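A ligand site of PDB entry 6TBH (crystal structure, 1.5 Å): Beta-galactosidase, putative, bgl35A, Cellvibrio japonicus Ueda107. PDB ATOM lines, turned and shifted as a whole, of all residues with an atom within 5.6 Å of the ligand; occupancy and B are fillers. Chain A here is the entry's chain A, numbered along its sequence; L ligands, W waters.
The side-chain carboxylate (OE1) of Glu 180 is in salt-bridge range of a nitrogen (N2) of the ligand (2.7 Å).
O3 of the ligand sits at hydrogen-bond distance from ND2 of Asn 358 (2.9 Å).
ND2 of Asn 110 lies within hydrogen-bond range of O4 of the ligand, at 2.9 Å.
The side-chain amino group (NZ) of Lys 109 sits at hydrogen-bond distance from an oxygen (O4) of the ligand (3.0 Å).
The side-chain amide nitrogen (ND2) of Asn 179 is in hydrogen-bond range of an oxygen (O5) of the ligand (3.1 Å).
The side-chain amide nitrogen of Asn 42 is in hydrogen-bond range of an oxygen (O5) of the ligand.
N of Phe 300 is in hydrogen-bond range of O1 of the ligand (3.3 Å).
N of Asn 110 is in hydrogen-bond range of O of Glu 180 (3.4 Å).
OE2 of Glu 180 sits close to OD2 of Asp 297 (2.4 Å).
N of Glu 180 lies within hydrogen-bond range of OD1 of Asn 256 (3.1 Å).
The side-chain amino group of Lys 109 sits at hydrogen-bond distance from the side-chain amide oxygen of Asn 110 (2.9 Å).
The side-chain amide nitrogen of Asn 256 lies within hydrogen-bond range of the side-chain amide oxygen of Asn 179 (3.0 Å).
OE1 of Glu 324 is in hydrogen-bond range of OH of Tyr 299 (2.7 Å).
The side-chain carboxylate of Glu 324 lies within hydrogen-bond range of the side-chain amide nitrogen of Asn 256.
The guanidinium group (NH2) of Arg 301 sits at hydrogen-bond distance from the backbone carbonyl oxygen (O) of Leu 361, 3.2 Å away.
The backbone carbonyl oxygen (O) of Tyr 299 sits close to an oxygen (O1) of the ligand, at 3.3 Å.
Glu 324 touches the ligand.
CZ of Phe 349 touches C3 of the ligand, at 3.5 Å.
CD1 of Leu 361 touches C5 of the ligand, at 3.7 Å.
Hydrophobic or aromatic side chains within 4 Å of the ligand: Tyr 299, Phe 300, Phe 349 and Leu 361.
11 residues have an atom within 4 Å of the ligand: Asn 42, Lys 109, Asn 110, Asn 179, Glu 180, Tyr 299, Phe 300, Glu 324, Phe 349, Asn 358 and Leu 361.
Water W2 bridges the side-chain amide nitrogen (ND2) of Asn 110 (3.0 Å) and a nitrogen (N2) of the ligand (3.1 Å).
Water W3 lies within hydrogen-bond range of the backbone NH (N) of Tyr 299 (2.8 Å), an oxygen (O1) of the ligand (3.3 Å) and the backbone NH (N) of Phe 300 (3.4 Å).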
ATOM      1  N   GLN A  39     -12.180  35.126  -9.129  1.00  0.00           N
ATOM      2  CA  GLN A  39     -11.223  34.233  -9.824  1.00  0.00           C
ATOM      3  C   GLN A  39     -10.330  35.140 -10.656  1.00  0.00           C
ATOM      4  O   GLN A  39     -10.779  35.986 -11.360  1.00  0.00           O
ATOM      5  CB  GLN A  39     -11.950  33.235 -10.682  1.00  0.00           C
ATOM      6  CG  GLN A  39     -11.022  32.276 -11.413  1.00  0.00           C
ATOM      7  CD  GLN A  39     -11.751  31.044 -11.816  1.00  0.00           C
ATOM      8  OE1 GLN A  39     -11.268  30.298 -12.562  1.00  0.00           O
ATOM      9  NE2 GLN A  39     -13.054  30.906 -11.424  1.00  0.00           N
ATOM     10  N   ASN A  42      -5.691  34.215 -16.018  1.00  0.00           N
ATOM     11  CA  ASN A  42      -4.887  32.995 -16.176  1.00  0.00           C
ATOM     12  C   ASN A  42      -3.380  33.217 -15.936  1.00  0.00           C
ATOM     13  O   ASN A  42      -2.685  32.224 -15.786  1.00  0.00           O
ATOM     14  CB  ASN A  42      -5.077  32.432 -17.567  1.00  0.00           C
ATOM     15  CG  ASN A  42      -6.370  31.677 -17.835  1.00  0.00           C
ATOM     16  OD1 ASN A  42      -6.625  31.447 -19.009  1.00  0.00           O
ATOM     17  ND2 ASN A  42      -7.178  31.324 -16.826  1.00  0.00           N
ATOM     18  N   PHE A 105      -3.511  23.483 -12.943  1.00  0.00           N
ATOM     19  CA  PHE A 105      -3.332  23.582 -14.390  1.00  0.00           C
ATOM     20  C   PHE A 105      -2.209  22.644 -14.781  1.00  0.00           C
ATOM     21  O   PHE A 105      -1.067  22.950 -14.434  1.00  0.00           O
ATOM     22  CB  PHE A 105      -3.018  25.038 -14.780  1.00  0.00           C
ATOM     23  CG  PHE A 105      -4.153  26.022 -14.797  1.00  0.00           C
ATOM     24  CD1 PHE A 105      -5.414  25.758 -14.229  1.00  0.00           C
ATOM     25  CD2 PHE A 105      -3.934  27.272 -15.341  1.00  0.00           C
ATOM     26  CE1 PHE A 105      -6.359  26.760 -14.228  1.00  0.00           C
ATOM     27  CE2 PHE A 105      -4.878  28.274 -15.316  1.00  0.00           C
ATOM     28  CZ  PHE A 105      -6.121  27.998 -14.772  1.00  0.00           C
ATOM     29  N   LYS A 109      -5.340  22.323 -19.687  1.00  0.00           N
ATOM     30  CA  LYS A 109      -5.818  23.680 -19.446  1.00  0.00           C
ATOM     31  C   LYS A 109      -6.474  24.058 -20.743  1.00  0.00           C
ATOM     32  O   LYS A 109      -5.773  24.323 -21.729  1.00  0.00           O
ATOM     33  CB  LYS A 109      -4.702  24.620 -18.904  1.00  0.00           C
ATOM     34  CG  LYS A 109      -5.195  25.914 -18.271  1.00  0.00           C
ATOM     35  CD  LYS A 109      -5.872  26.841 -19.285  1.00  0.00           C
ATOM     36  CE  LYS A 109      -6.270  28.196 -18.740  1.00  0.00           C
ATOM     37  NZ  LYS A 109      -7.173  28.851 -19.704  1.00  0.00           N
ATOM     38  N   ASN A 110      -7.808  24.156 -20.769  1.00  0.00           N
ATOM     39  CA  ASN A 110      -8.536  24.463 -22.020  1.00  0.00           C
ATOM     40  C   ASN A 110      -8.056  23.507 -23.103  1.00  0.00           C
ATOM     41  O   ASN A 110      -7.744  23.977 -24.196  1.00  0.00           O
ATOM     42  CB  ASN A 110      -8.438  25.934 -22.423  1.00  0.00           C
ATOM     43  CG  ASN A 110      -9.038  26.944 -21.453  1.00  0.00           C
ATOM     44  OD1 ASN A 110      -9.090  26.711 -20.244  1.00  0.00           O
ATOM     45  ND2 ASN A 110      -9.413  28.101 -22.006  1.00  0.00           N
ATOM     46  N   ASN A 179      -8.147  21.994 -15.797  1.00  0.00           N
ATOM     47  CA  ASN A 179      -8.988  23.188 -16.112  1.00  0.00           C
ATOM     48  C   ASN A 179      -9.582  22.963 -17.483  1.00  0.00           C
ATOM     49  O   ASN A 179      -8.834  22.970 -18.501  1.00  0.00           O
ATOM     50  CB  ASN A 179      -8.204  24.514 -16.022  1.00  0.00           C
ATOM     51  CG  ASN A 179      -9.033  25.743 -16.235  1.00  0.00           C
ATOM     52  OD1 ASN A 179      -9.589  26.246 -15.255  1.00  0.00           O
ATOM     53  ND2 ASN A 179      -9.135  26.239 -17.481  1.00  0.00           N
ATOM     54  N   GLU A 180     -10.916  22.806 -17.568  1.00  0.00           N
ATOM     55  CA  GLU A 180     -11.591  22.607 -18.866  1.00  0.00           C
ATOM     56  C   GLU A 180     -10.863  21.523 -19.702  1.00  0.00           C
ATOM     57  O   GLU A 180     -10.305  21.796 -20.769  1.00  0.00           O
ATOM     58  CB  GLU A 180     -11.780  23.913 -19.644  1.00  0.00           C
ATOM     59  CG  GLU A 180     -12.726  24.871 -18.961  1.00  0.00           C
ATOM     60  CD  GLU A 180     -13.208  26.084 -19.751  1.00  0.00           C
ATOM     61  OE1 GLU A 180     -12.598  26.419 -20.811  1.00  0.00           O
ATOM     62  OE2 GLU A 180     -14.182  26.772 -19.257  1.00  0.00           O
ATOM     63  N   TYR A 184     -10.418  20.013 -28.547  1.00  0.00           N
ATOM     64  CA  TYR A 184     -10.981  20.739 -29.697  1.00  0.00           C
ATOM     65  C   TYR A 184     -10.414  20.135 -30.968  1.00  0.00           C
ATOM     66  O   TYR A 184      -9.180  19.844 -31.030  1.00  0.00           O
ATOM     67  CB  TYR A 184     -10.681  22.217 -29.588  1.00  0.00           C
ATOM     68  CG  TYR A 184     -11.363  22.939 -28.451  1.00  0.00           C
ATOM     69  CD1 TYR A 184     -12.720  23.163 -28.467  1.00  0.00           C
ATOM     70  CD2 TYR A 184     -10.658  23.470 -27.372  1.00  0.00           C
ATOM     71  CE1 TYR A 184     -13.347  23.878 -27.446  1.00  0.00           C
ATOM     72  CE2 TYR A 184     -11.254  24.167 -26.323  1.00  0.00           C
ATOM     73  CZ  TYR A 184     -12.639  24.317 -26.364  1.00  0.00           C
ATOM     74  OH  TYR A 184     -13.321  25.021 -25.427  1.00  0.00           O
ATOM     75  N   ASN A 256     -14.078  21.465 -13.863  1.00  0.00           N
ATOM     76  CA  ASN A 256     -14.814  22.616 -14.444  1.00  0.00           C
ATOM     77  C   ASN A 256     -14.971  22.398 -15.931  1.00  0.00           C
ATOM     78  O   ASN A 256     -14.002  22.140 -16.699  1.00  0.00           O
ATOM     79  CB  ASN A 256     -14.156  23.954 -14.120  1.00  0.00           C
ATOM     80  CG  ASN A 256     -12.785  24.068 -14.788  1.00  0.00           C
ATOM     81  OD1 ASN A 256     -11.973  23.165 -14.669  1.00  0.00           O
ATOM     82  ND2 ASN A 256     -12.470  25.269 -15.237  1.00  0.00           N
ATOM     83  N   ALA A 258     -15.876  23.297 -19.846  1.00  0.00           N
ATOM     84  CA  ALA A 258     -16.131  24.125 -21.047  1.00  0.00           C
ATOM     85  C   ALA A 258     -17.445  23.628 -21.680  1.00  0.00           C
ATOM     86  O   ALA A 258     -17.461  22.605 -22.346  1.00  0.00           O
ATOM     87  CB  ALA A 258     -14.975  24.015 -21.991  1.00  0.00           C
ATOM     88  N   LEU A 259     -18.506  24.367 -21.387  1.00  0.00           N
ATOM     89  CA  LEU A 259     -19.873  23.933 -21.707  1.00  0.00           C
ATOM     90  C   LEU A 259     -20.069  23.818 -23.196  1.00  0.00           C
ATOM     91  O   LEU A 259     -19.586  24.657 -23.990  1.00  0.00           O
ATOM     92  CB  LEU A 259     -20.873  24.922 -21.124  1.00  0.00           C
ATOM     93  CG  LEU A 259     -20.820  25.030 -19.601  1.00  0.00           C
ATOM     94  CD1 LEU A 259     -21.804  26.072 -19.096  1.00  0.00           C
ATOM     95  CD2 LEU A 259     -21.068  23.668 -18.865  1.00  0.00           C
ATOM     96  N   ASN A 261     -23.394  24.237 -25.716  1.00  0.00           N
ATOM     97  CA  ASN A 261     -24.719  24.911 -25.708  1.00  0.00           C
ATOM     98  C   ASN A 261     -25.740  23.799 -25.470  1.00  0.00           C
ATOM     99  O   ASN A 261     -25.776  22.832 -26.225  1.00  0.00           O
ATOM    100  CB  ASN A 261     -24.965  25.684 -26.976  1.00  0.00           C
ATOM    101  CG  ASN A 261     -26.262  26.445 -26.895  1.00  0.00           C
ATOM    102  OD1 ASN A 261     -27.349  25.854 -26.764  1.00  0.00           O
ATOM    103  ND2 ASN A 261     -26.188  27.753 -26.955  1.00  0.00           N
ATOM    104  N   ASP A 297     -18.783  26.161 -16.365  1.00  0.00           N
ATOM    105  CA  ASP A 297     -18.129  27.464 -16.613  1.00  0.00           C
ATOM    106  C   ASP A 297     -19.060  28.230 -17.550  1.00  0.00           C
ATOM    107  O   ASP A 297     -19.199  27.876 -18.717  1.00  0.00           O
ATOM    108  CB  ASP A 297     -16.746  27.280 -17.260  1.00  0.00           C
ATOM    109  CG  ASP A 297     -15.693  26.675 -16.362  1.00  0.00           C
ATOM    110  OD1 ASP A 297     -15.929  26.594 -15.162  1.00  0.00           O
ATOM    111  OD2 ASP A 297     -14.613  26.303 -16.893  1.00  0.00           O
ATOM    112  N   TYR A 299     -20.568  31.215 -19.706  1.00  0.00           N
ATOM    113  CA  TYR A 299     -20.293  32.460 -20.480  1.00  0.00           C
ATOM    114  C   TYR A 299     -21.452  32.764 -21.430  1.00  0.00           C
ATOM    115  O   TYR A 299     -21.412  33.778 -22.137  1.00  0.00           O
ATOM    116  CB  TYR A 299     -18.973  32.406 -21.250  1.00  0.00           C
ATOM    117  CG  TYR A 299     -17.790  32.331 -20.307  1.00  0.00           C
ATOM    118  CD1 TYR A 299     -17.374  33.436 -19.573  1.00  0.00           C
ATOM    119  CD2 TYR A 299     -17.291  31.096 -19.944  1.00  0.00           C
ATOM    120  CE1 TYR A 299     -16.318  33.335 -18.683  1.00  0.00           C
ATOM    121  CE2 TYR A 299     -16.220  30.962 -19.051  1.00  0.00           C
ATOM    122  CZ  TYR A 299     -15.728  32.089 -18.400  1.00  0.00           C
ATOM    123  OH  TYR A 299     -14.697  32.071 -17.484  1.00  0.00           O
ATOM    124  N   PHE A 300     -22.520  31.955 -21.363  1.00  0.00           N
ATOM    125  CA  PHE A 300     -23.746  32.293 -22.138  1.00  0.00           C
ATOM    126  C   PHE A 300     -24.411  33.520 -21.447  1.00  0.00           C
ATOM    127  O   PHE A 300     -24.452  33.530 -20.236  1.00  0.00           O
ATOM    128  CB  PHE A 300     -24.722  31.125 -22.119  1.00  0.00           C
ATOM    129  CG  PHE A 300     -24.189  29.790 -22.566  1.00  0.00           C
ATOM    130  CD1 PHE A 300     -23.724  29.574 -23.847  1.00  0.00           C
ATOM    131  CD2 PHE A 300     -24.079  28.738 -21.681  1.00  0.00           C
ATOM    132  CE1 PHE A 300     -23.228  28.341 -24.247  1.00  0.00           C
ATOM    133  CE2 PHE A 300     -23.618  27.502 -22.080  1.00  0.00           C
ATOM    134  CZ  PHE A 300     -23.156  27.314 -23.360  1.00  0.00           C
ATOM    135  N   ARG A 301     -24.815  34.570 -22.134  1.00  0.00           N
ATOM    136  CA  ARG A 301     -25.322  35.754 -21.358  1.00  0.00           C
ATOM    137  C   ARG A 301     -26.825  35.698 -21.171  1.00  0.00           C
ATOM    138  O   ARG A 301     -27.313  36.305 -20.111  1.00  0.00           O
ATOM    139  CB  ARG A 301     -25.042  37.104 -22.030  1.00  0.00           C
ATOM    140  CG  ARG A 301     -23.588  37.515 -21.962  1.00  0.00           C
ATOM    141  CD  ARG A 301     -22.953  37.863 -23.305  1.00  0.00           C
ATOM    142  NE  ARG A 301     -21.589  38.312 -23.034  1.00  0.00           N
ATOM    143  CZ  ARG A 301     -21.289  39.471 -22.479  1.00  0.00           C
ATOM    144  NH1 ARG A 301     -22.234  40.305 -22.091  1.00  0.00           N
ATOM    145  NH2 ARG A 301     -20.022  39.769 -22.263  1.00  0.00           N
ATOM    146  N   GLU A 324     -16.835  29.098 -12.783  1.00  0.00           N
ATOM    147  CA  GLU A 324     -16.528  30.324 -13.531  1.00  0.00           C
ATOM    148  C   GLU A 324     -17.844  30.913 -14.027  1.00  0.00           C
ATOM    149  O   GLU A 324     -18.722  30.159 -14.522  1.00  0.00           O
ATOM    150  CB  GLU A 324     -15.627  30.065 -14.761  1.00  0.00           C
ATOM    151  CG  GLU A 324     -14.324  29.491 -14.444  1.00  0.00           C
ATOM    152  CD  GLU A 324     -13.513  29.138 -15.689  1.00  0.00           C
ATOM    153  OE1 GLU A 324     -13.834  29.610 -16.756  1.00  0.00           O
ATOM    154  OE2 GLU A 324     -12.518  28.337 -15.502  1.00  0.00           O
ATOM    155  N   PHE A 349     -15.133  35.260 -13.306  1.00  0.00           N
ATOM    156  CA  PHE A 349     -13.787  35.064 -13.874  1.00  0.00           C
ATOM    157  C   PHE A 349     -13.195  36.405 -14.291  1.00  0.00           C
ATOM    158  O   PHE A 349     -13.831  37.148 -14.998  1.00  0.00           O
ATOM    159  CB  PHE A 349     -13.875  34.125 -15.068  1.00  0.00           C
ATOM    160  CG  PHE A 349     -12.530  33.879 -15.656  1.00  0.00           C
ATOM    161  CD1 PHE A 349     -11.750  32.834 -15.166  1.00  0.00           C
ATOM    162  CD2 PHE A 349     -12.057  34.698 -16.642  1.00  0.00           C
ATOM    163  CE1 PHE A 349     -10.457  32.624 -15.654  1.00  0.00           C
ATOM    164  CE2 PHE A 349     -10.786  34.458 -17.162  1.00  0.00           C
ATOM    165  CZ  PHE A 349     -10.037  33.431 -16.675  1.00  0.00           C
ATOM    166  N   ASN A 358     -11.415  39.319 -21.002  1.00  0.00           N
ATOM    167  CA  ASN A 358     -11.767  38.209 -21.911  1.00  0.00           C
ATOM    168  C   ASN A 358     -13.034  38.543 -22.717  1.00  0.00           C
ATOM    169  O   ASN A 358     -13.578  37.639 -23.381  1.00  0.00           O
ATOM    170  CB  ASN A 358     -11.849  36.870 -21.176  1.00  0.00           C
ATOM    171  CG  ASN A 358     -13.063  36.776 -20.265  1.00  0.00           C
ATOM    172  OD1 ASN A 358     -13.733  37.788 -20.020  1.00  0.00           O
ATOM    173  ND2 ASN A 358     -13.300  35.582 -19.761  1.00  0.00           N
ATOM    174  N   LEU A 361     -16.341  37.370 -23.985  1.00  0.00           N
ATOM    175  CA  LEU A 361     -16.921  36.491 -22.927  1.00  0.00           C
ATOM    176  C   LEU A 361     -17.300  37.348 -21.713  1.00  0.00           C
ATOM    177  O   LEU A 361     -18.409  37.177 -21.178  1.00  0.00           O
ATOM    178  CB  LEU A 361     -15.922  35.439 -22.502  1.00  0.00           C
ATOM    179  CG  LEU A 361     -15.533  34.417 -23.574  1.00  0.00           C
ATOM    180  CD1 LEU A 361     -14.788  33.316 -22.915  1.00  0.00           C
ATOM    181  CD2 LEU A 361     -16.728  33.898 -24.346  1.00  0.00           C
HETATM  182  C1  LIG L   1     -12.488  29.734 -19.653  1.00  0.00           C
HETATM  183  C2  LIG L   1     -11.846  31.152 -19.585  1.00  0.00           C
HETATM  184  O1  LIG L   1     -20.816  31.310 -24.169  1.00  0.00           O
HETATM  185  C3  LIG L   1     -10.425  30.915 -19.090  1.00  0.00           C
HETATM  186  C4  LIG L   1     -21.822  30.487 -26.397  1.00  0.00           C
HETATM  187  C5  LIG L   1     -12.067  32.062 -20.742  1.00  0.00           C
HETATM  188  C6  LIG L   1     -13.910  29.528 -21.628  1.00  0.00           C
HETATM  189  S1  LIG L   1     -20.585  31.080 -25.536  1.00  0.00           S
HETATM  190  O2  LIG L   1     -20.213  32.437 -26.064  1.00  0.00           O
HETATM  191  N1  LIG L   1     -19.467  29.932 -25.646  1.00  0.00           N
HETATM  192  C7  LIG L   1     -18.230  30.342 -24.975  1.00  0.00           C
HETATM  193  C8  LIG L   1     -17.659  29.125 -24.303  1.00  0.00           C
HETATM  194  C9  LIG L   1     -16.144  28.936 -24.660  1.00  0.00           C
HETATM  195  C10 LIG L   1     -15.358  29.532 -23.583  1.00  0.00           C
HETATM  196  C11 LIG L   1     -14.122  28.849 -22.971  1.00  0.00           C
HETATM  197  N2  LIG L   1     -12.609  29.142 -20.994  1.00  0.00           N
HETATM  198  C12 LIG L   1     -11.476  28.863 -18.859  1.00  0.00           C
HETATM  199  O3  LIG L   1     -11.575  33.370 -20.429  1.00  0.00           O
HETATM  200  O4  LIG L   1      -9.701  30.374 -20.182  1.00  0.00           O
HETATM  201  C13 LIG L   1     -10.633  29.831 -18.087  1.00  0.00           C
HETATM  202  O5  LIG L   1      -9.435  29.273 -17.578  1.00  0.00           O
HETATM  203  O   HOH W   1      -9.496  29.141 -14.787  1.00  0.00           O
HETATM  204  O   HOH W   2     -11.117  30.050 -23.510  1.00  0.00           O
HETATM  205  O   HOH W   3     -20.600  29.190 -21.667  1.00  0.00           O
